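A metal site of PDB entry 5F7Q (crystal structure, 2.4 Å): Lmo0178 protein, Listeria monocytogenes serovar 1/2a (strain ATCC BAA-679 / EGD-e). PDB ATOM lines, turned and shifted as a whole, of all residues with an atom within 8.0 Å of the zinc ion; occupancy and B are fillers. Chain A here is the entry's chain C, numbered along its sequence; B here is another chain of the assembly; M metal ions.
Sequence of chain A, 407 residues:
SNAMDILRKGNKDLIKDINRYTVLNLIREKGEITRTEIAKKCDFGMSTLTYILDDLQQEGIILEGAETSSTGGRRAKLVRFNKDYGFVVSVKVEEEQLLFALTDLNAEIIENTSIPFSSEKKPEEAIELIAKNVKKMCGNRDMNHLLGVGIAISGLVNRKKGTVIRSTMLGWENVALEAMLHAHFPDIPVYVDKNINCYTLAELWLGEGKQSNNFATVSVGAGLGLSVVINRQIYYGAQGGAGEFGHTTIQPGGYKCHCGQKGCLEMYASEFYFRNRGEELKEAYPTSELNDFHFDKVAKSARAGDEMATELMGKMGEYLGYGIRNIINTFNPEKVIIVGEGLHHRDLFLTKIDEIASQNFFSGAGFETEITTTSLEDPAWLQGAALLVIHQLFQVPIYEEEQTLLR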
ATOM      1  N   ARG A 166      19.469 -34.773  -3.648  1.00  0.00           N
ATOM      2  CA  ARG A 166      20.555 -34.318  -2.778  1.00  0.00           C
ATOM      3  C   ARG A 166      20.061 -34.135  -1.370  1.00  0.00           C
ATOM      4  O   ARG A 166      18.948 -33.710  -1.173  1.00  0.00           O
ATOM      5  CB  ARG A 166      21.090 -32.977  -3.259  1.00  0.00           C
ATOM      6  CG  ARG A 166      22.340 -32.500  -2.524  1.00  0.00           C
ATOM      7  CD  ARG A 166      22.781 -31.151  -3.077  1.00  0.00           C
ATOM      8  NE  ARG A 166      21.876 -30.079  -2.671  1.00  0.00           N
ATOM      9  CZ  ARG A 166      21.722 -28.929  -3.297  1.00  0.00           C
ATOM     10  NH1 ARG A 166      22.378 -28.660  -4.427  1.00  0.00           N
ATOM     11  NH2 ARG A 166      20.880 -28.028  -2.824  1.00  0.00           N
ATOM     12  N   GLU A 244      11.517 -23.911  -3.031  1.00  0.00           N
ATOM     13  CA  GLU A 244      12.454 -23.759  -1.934  1.00  0.00           C
ATOM     14  C   GLU A 244      12.539 -22.317  -1.449  1.00  0.00           C
ATOM     15  O   GLU A 244      13.529 -21.619  -1.675  1.00  0.00           O
ATOM     16  CB  GLU A 244      13.835 -24.253  -2.375  1.00  0.00           C
ATOM     17  CG  GLU A 244      13.912 -25.758  -2.611  1.00  0.00           C
ATOM     18  CD  GLU A 244      13.851 -26.575  -1.334  1.00  0.00           C
ATOM     19  OE1 GLU A 244      14.000 -26.003  -0.230  1.00  0.00           O
ATOM     20  OE2 GLU A 244      13.669 -27.819  -1.423  1.00  0.00           O
ATOM     21  N   PHE A 245      11.503 -21.891  -0.722  1.00  0.00           N
ATOM     22  CA  PHE A 245      11.425 -20.547  -0.175  1.00  0.00           C
ATOM     23  C   PHE A 245      12.553 -20.241   0.796  1.00  0.00           C
ATOM     24  O   PHE A 245      13.012 -19.102   0.885  1.00  0.00           O
ATOM     25  CB  PHE A 245      10.096 -20.340   0.513  1.00  0.00           C
ATOM     26  CG  PHE A 245       9.765 -18.919   0.709  1.00  0.00           C
ATOM     27  CD1 PHE A 245       9.253 -18.177  -0.344  1.00  0.00           C
ATOM     28  CD2 PHE A 245       9.976 -18.293   1.922  1.00  0.00           C
ATOM     29  CE1 PHE A 245       8.951 -16.834  -0.204  1.00  0.00           C
ATOM     30  CE2 PHE A 245       9.703 -16.941   2.067  1.00  0.00           C
ATOM     31  CZ  PHE A 245       9.184 -16.212   1.013  1.00  0.00           C
ATOM     32  N   GLY A 246      13.033 -21.250   1.510  1.00  0.00           N
ATOM     33  CA  GLY A 246      14.144 -21.043   2.420  1.00  0.00           C
ATOM     34  C   GLY A 246      15.406 -20.552   1.702  1.00  0.00           C
ATOM     35  O   GLY A 246      16.263 -19.884   2.309  1.00  0.00           O
ATOM     36  N   HIS A 247      15.488 -20.837   0.409  1.00  0.00           N
ATOM     37  CA  HIS A 247      16.620 -20.459  -0.422  1.00  0.00           C
ATOM     38  C   HIS A 247      16.334 -19.324  -1.423  1.00  0.00           C
ATOM     39  O   HIS A 247      16.943 -19.242  -2.495  1.00  0.00           O
ATOM     40  CB  HIS A 247      17.229 -21.726  -1.077  1.00  0.00           C
ATOM     41  CG  HIS A 247      17.627 -22.763  -0.077  1.00  0.00           C
ATOM     42  ND1 HIS A 247      18.804 -22.716   0.620  1.00  0.00           N
ATOM     43  CD2 HIS A 247      16.951 -23.835   0.399  1.00  0.00           C
ATOM     44  CE1 HIS A 247      18.872 -23.744   1.449  1.00  0.00           C
ATOM     45  NE2 HIS A 247      17.758 -24.437   1.349  1.00  0.00           N
ATOM     46  N   THR A 248      15.425 -18.433  -1.034  1.00  0.00           N
ATOM     47  CA  THR A 248      15.188 -17.201  -1.792  1.00  0.00           C
ATOM     48  C   THR A 248      16.262 -16.253  -1.283  1.00  0.00           C
ATOM     49  O   THR A 248      16.629 -16.305  -0.098  1.00  0.00           O
ATOM     50  CB  THR A 248      13.805 -16.608  -1.488  1.00  0.00           C
ATOM     51  OG1 THR A 248      13.552 -16.673  -0.078  1.00  0.00           O
ATOM     52  CG2 THR A 248      12.714 -17.383  -2.221  1.00  0.00           C
ATOM     53  N   THR A 249      16.777 -15.395  -2.153  1.00  0.00           N
ATOM     54  CA  THR A 249      17.803 -14.435  -1.748  1.00  0.00           C
ATOM     55  C   THR A 249      17.228 -13.254  -0.981  1.00  0.00           C
ATOM     56  O   THR A 249      16.317 -12.591  -1.477  1.00  0.00           O
ATOM     57  CB  THR A 249      18.512 -13.843  -2.995  1.00  0.00           C
ATOM     58  OG1 THR A 249      19.116 -14.892  -3.754  1.00  0.00           O
ATOM     59  CG2 THR A 249      19.580 -12.835  -2.599  1.00  0.00           C
ATOM     60  N   TYR A 255      25.550 -14.266   3.502  1.00  0.00           N
ATOM     61  CA  TYR A 255      26.177 -15.494   3.989  1.00  0.00           C
ATOM     62  C   TYR A 255      26.123 -16.630   2.983  1.00  0.00           C
ATOM     63  O   TYR A 255      25.073 -16.937   2.420  1.00  0.00           O
ATOM     64  CB  TYR A 255      25.558 -15.999   5.314  1.00  0.00           C
ATOM     65  CG  TYR A 255      25.704 -15.034   6.465  1.00  0.00           C
ATOM     66  CD1 TYR A 255      26.963 -14.649   6.916  1.00  0.00           C
ATOM     67  CD2 TYR A 255      24.581 -14.547   7.125  1.00  0.00           C
ATOM     68  CE1 TYR A 255      27.101 -13.756   7.972  1.00  0.00           C
ATOM     69  CE2 TYR A 255      24.702 -13.676   8.191  1.00  0.00           C
ATOM     70  CZ  TYR A 255      25.951 -13.277   8.618  1.00  0.00           C
ATOM     71  OH  TYR A 255      26.041 -12.404   9.678  1.00  0.00           O
ATOM     72  N   LYS A 256      27.263 -17.246   2.788  1.00  0.00           N
ATOM     73  CA  LYS A 256      27.360 -18.357   1.903  1.00  0.00           C
ATOM     74  C   LYS A 256      26.451 -19.442   2.477  1.00  0.00           C
ATOM     75  O   LYS A 256      26.577 -19.818   3.659  1.00  0.00           O
ATOM     76  CB  LYS A 256      28.814 -18.857   1.848  1.00  0.00           C
ATOM     77  CG  LYS A 256      29.238 -19.478   0.518  1.00  0.00           C
ATOM     78  CD  LYS A 256      28.376 -20.632   0.051  1.00  0.00           C
ATOM     79  CE  LYS A 256      28.808 -21.093  -1.321  1.00  0.00           C
ATOM     80  NZ  LYS A 256      30.226 -21.545  -1.359  1.00  0.00           N
ATOM     81  N   CYS A 257      25.549 -19.952   1.653  1.00  0.00           N
ATOM     82  CA  CYS A 257      24.646 -21.017   2.041  1.00  0.00           C
ATOM     83  C   CYS A 257      25.146 -22.373   1.489  1.00  0.00           C
ATOM     84  O   CYS A 257      25.883 -22.402   0.510  1.00  0.00           O
ATOM     85  CB  CYS A 257      23.250 -20.695   1.525  1.00  0.00           C
ATOM     86  SG  CYS A 257      21.967 -21.900   1.895  1.00  0.00           S
ATOM     87  N   HIS A 258      24.770 -23.478   2.155  1.00  0.00           N
ATOM     88  CA  HIS A 258      25.102 -24.845   1.684  1.00  0.00           C
ATOM     89  C   HIS A 258      24.473 -25.191   0.295  1.00  0.00           C
ATOM     90  O   HIS A 258      24.922 -26.143  -0.376  1.00  0.00           O
ATOM     91  CB  HIS A 258      24.709 -25.900   2.751  1.00  0.00           C
ATOM     92  CG  HIS A 258      23.286 -25.796   3.218  1.00  0.00           C
ATOM     93  ND1 HIS A 258      22.255 -26.505   2.653  1.00  0.00           N
ATOM     94  CD2 HIS A 258      22.719 -25.025   4.178  1.00  0.00           C
ATOM     95  CE1 HIS A 258      21.112 -26.182   3.239  1.00  0.00           C
ATOM     96  NE2 HIS A 258      21.376 -25.284   4.166  1.00  0.00           N
ATOM     97  N   CYS A 259      23.459 -24.446  -0.141  1.00  0.00           N
ATOM     98  CA  CYS A 259      22.877 -24.672  -1.496  1.00  0.00           C
ATOM     99  C   CYS A 259      23.768 -24.116  -2.649  1.00  0.00           C
ATOM    100  O   CYS A 259      23.478 -24.328  -3.832  1.00  0.00           O
ATOM    101  CB  CYS A 259      21.493 -24.034  -1.621  1.00  0.00           C
ATOM    102  SG  CYS A 259      21.448 -22.239  -1.821  1.00  0.00           S
ATOM    103  N   GLY A 260      24.830 -23.379  -2.308  1.00  0.00           N
ATOM    104  CA  GLY A 260      25.722 -22.772  -3.303  1.00  0.00           C
ATOM    105  C   GLY A 260      25.453 -21.296  -3.556  1.00  0.00           C
ATOM    106  O   GLY A 260      26.260 -20.623  -4.145  1.00  0.00           O
ATOM    107  N   GLN A 261      24.320 -20.790  -3.117  1.00  0.00           N
ATOM    108  CA  GLN A 261      23.991 -19.375  -3.290  1.00  0.00           C
ATOM    109  C   GLN A 261      24.513 -18.559  -2.103  1.00  0.00           C
ATOM    110  O   GLN A 261      24.888 -19.125  -1.061  1.00  0.00           O
ATOM    111  CB  GLN A 261      22.456 -19.168  -3.366  1.00  0.00           C
ATOM    112  CG  GLN A 261      21.724 -19.764  -4.575  1.00  0.00           C
ATOM    113  CD  GLN A 261      20.212 -19.486  -4.522  1.00  0.00           C
ATOM    114  OE1 GLN A 261      19.702 -18.692  -5.295  1.00  0.00           O
ATOM    115  NE2 GLN A 261      19.513 -20.122  -3.576  1.00  0.00           N
ATOM    116  N   LYS A 262      24.528 -17.241  -2.254  1.00  0.00           N
ATOM    117  CA  LYS A 262      24.878 -16.344  -1.155  1.00  0.00           C
ATOM    118  C   LYS A 262      23.618 -15.585  -0.716  1.00  0.00           C
ATOM    119  O   LYS A 262      22.814 -15.207  -1.531  1.00  0.00           O
ATOM    120  CB  LYS A 262      25.964 -15.350  -1.588  1.00  0.00           C
ATOM    121  CG  LYS A 262      27.308 -16.010  -1.869  1.00  0.00           C
ATOM    122  CD  LYS A 262      28.458 -14.993  -1.972  1.00  0.00           C
ATOM    123  CE  LYS A 262      29.797 -15.688  -2.105  1.00  0.00           C
ATOM    124  NZ  LYS A 262      30.924 -14.707  -2.208  1.00  0.00           N
ATOM    125  N   GLY A 263      23.461 -15.378   0.583  1.00  0.00           N
ATOM    126  CA  GLY A 263      22.352 -14.569   1.108  1.00  0.00           C
ATOM    127  C   GLY A 263      20.950 -15.173   1.215  1.00  0.00           C
ATOM    128  O   GLY A 263      19.983 -14.433   1.253  1.00  0.00           O
ATOM    129  N   CYS A 264      20.841 -16.484   1.294  1.00  0.00           N
ATOM    130  CA  CYS A 264      19.521 -17.113   1.391  1.00  0.00           C
ATOM    131  C   CYS A 264      18.775 -16.751   2.661  1.00  0.00           C
ATOM    132  O   CYS A 264      19.377 -16.526   3.711  1.00  0.00           O
ATOM    133  CB  CYS A 264      19.647 -18.631   1.311  1.00  0.00           C
ATOM    134  SG  CYS A 264      20.271 -19.254  -0.267  1.00  0.00           S
ATOM    135  N   LEU A 265      17.463 -16.699   2.550  1.00  0.00           N
ATOM    136  CA  LEU A 265      16.595 -16.421   3.683  1.00  0.00           C
ATOM    137  C   LEU A 265      16.945 -17.276   4.936  1.00  0.00           C
ATOM    138  O   LEU A 265      17.070 -16.722   6.027  1.00  0.00           O
ATOM    139  CB  LEU A 265      15.130 -16.693   3.298  1.00  0.00           C
ATOM    140  CG  LEU A 265      14.044 -16.490   4.345  1.00  0.00           C
ATOM    141  CD1 LEU A 265      14.028 -15.084   4.927  1.00  0.00           C
ATOM    142  CD2 LEU A 265      12.707 -16.812   3.705  1.00  0.00           C
ATOM    143  N   GLU A 266      17.129 -18.589   4.767  1.00  0.00           N
ATOM    144  CA  GLU A 266      17.377 -19.432   5.925  1.00  0.00           C
ATOM    145  C   GLU A 266      18.706 -19.195   6.617  1.00  0.00           C
ATOM    146  O   GLU A 266      18.940 -19.691   7.704  1.00  0.00           O
ATOM    147  CB  GLU A 266      17.171 -20.922   5.608  1.00  0.00           C
ATOM    148  CG  GLU A 266      18.233 -21.614   4.759  1.00  0.00           C
ATOM    149  CD  GLU A 266      17.943 -23.090   4.670  1.00  0.00           C
ATOM    150  OE1 GLU A 266      18.877 -23.898   4.810  1.00  0.00           O
ATOM    151  OE2 GLU A 266      16.744 -23.432   4.545  1.00  0.00           O
ATOM    152  N   MET A 267      19.580 -18.423   5.977  1.00  0.00           N
ATOM    153  CA  MET A 267      20.840 -18.045   6.614  1.00  0.00           C
ATOM    154  C   MET A 267      20.595 -16.866   7.593  1.00  0.00           C
ATOM    155  O   MET A 267      21.483 -16.498   8.342  1.00  0.00           O
ATOM    156  CB  MET A 267      21.866 -17.630   5.550  1.00  0.00           C
ATOM    157  CG  MET A 267      22.365 -18.741   4.634  1.00  0.00           C
ATOM    158  SD  MET A 267      23.349 -20.002   5.466  1.00  0.00           S
ATOM    159  CE  MET A 267      22.098 -21.184   5.922  1.00  0.00           C
ATOM    160  N   ASN B 329      13.459 -19.760  -7.267  1.00  0.00           N
ATOM    161  CA  ASN B 329      13.683 -20.471  -6.040  1.00  0.00           C
ATOM    162  C   ASN B 329      12.374 -20.849  -5.337  1.00  0.00           C
ATOM    163  O   ASN B 329      12.253 -21.938  -4.776  1.00  0.00           O
ATOM    164  CB  ASN B 329      14.570 -19.634  -5.120  1.00  0.00           C
ATOM    165  CG  ASN B 329      15.982 -19.425  -5.685  1.00  0.00           C
ATOM    166  OD1 ASN B 329      16.492 -20.265  -6.390  1.00  0.00           O
ATOM    167  ND2 ASN B 329      16.616 -18.316  -5.351  1.00  0.00           N
ATOM    168  N   ASN B 360      20.791 -19.802  -9.202  1.00  0.00           N
ATOM    169  CA  ASN B 360      19.666 -20.017  -8.289  1.00  0.00           C
ATOM    170  C   ASN B 360      19.808 -21.375  -7.585  1.00  0.00           C
ATOM    171  O   ASN B 360      20.752 -22.111  -7.855  1.00  0.00           O
ATOM    172  CB  ASN B 360      18.306 -19.861  -9.012  1.00  0.00           C
ATOM    173  CG  ASN B 360      18.134 -20.843 -10.166  1.00  0.00           C
ATOM    174  OD1 ASN B 360      18.033 -22.066  -9.963  1.00  0.00           O
ATOM    175  ND2 ASN B 360      18.049 -20.309 -11.392  1.00  0.00           N
ATOM    176  N   PHE B 361      18.867 -21.687  -6.683  1.00  0.00           N
ATOM    177  CA  PHE B 361      18.923 -22.916  -5.911  1.00  0.00           C
ATOM    178  C   PHE B 361      18.984 -24.146  -6.777  1.00  0.00           C
ATOM    179  O   PHE B 361      19.804 -25.031  -6.526  1.00  0.00           O
ATOM    180  CB  PHE B 361      17.727 -23.036  -4.964  1.00  0.00           C
ATOM    181  CG  PHE B 361      17.681 -24.344  -4.213  1.00  0.00           C
ATOM    182  CD1 PHE B 361      18.341 -24.485  -3.017  1.00  0.00           C
ATOM    183  CD2 PHE B 361      16.997 -25.424  -4.726  1.00  0.00           C
ATOM    184  CE1 PHE B 361      18.306 -25.683  -2.310  1.00  0.00           C
ATOM    185  CE2 PHE B 361      16.968 -26.627  -4.048  1.00  0.00           C
ATOM    186  CZ  PHE B 361      17.633 -26.763  -2.832  1.00  0.00           C
HETATM  187 ZN    ZN M   1      20.480 -21.513   0.156  1.00  0.00          ZN
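NE2 of His 247 lies within hydrogen-bond range of OE2 of Glu 266 (3.5 Å). NE2 of Gln 261 lies close to SG of Cys 259. O of His 247 lies within hydrogen-bond range of NE2 of Gln 261 (2.9 Å). The side-chain amide nitrogen of Asn 329 of chain B is in hydrogen-bond range of the backbone carbonyl oxygen of His 247. The side-chain sulfur of Cys 264 sits close to the side-chain amide nitrogen of Gln 261 (3.5 Å).
The nearest printed residue that does not touch the zinc ion is Gln 261 (4.1 Å).
The zinc ion is bound by ND1 of His 247 (2.1 Å), SG of Cys 264 (2.3 Å), SG of Cys 259 (2.3 Å) and SG of Cys 257 (2.3 Å). The zinc ion has four donor atoms within binding distance.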
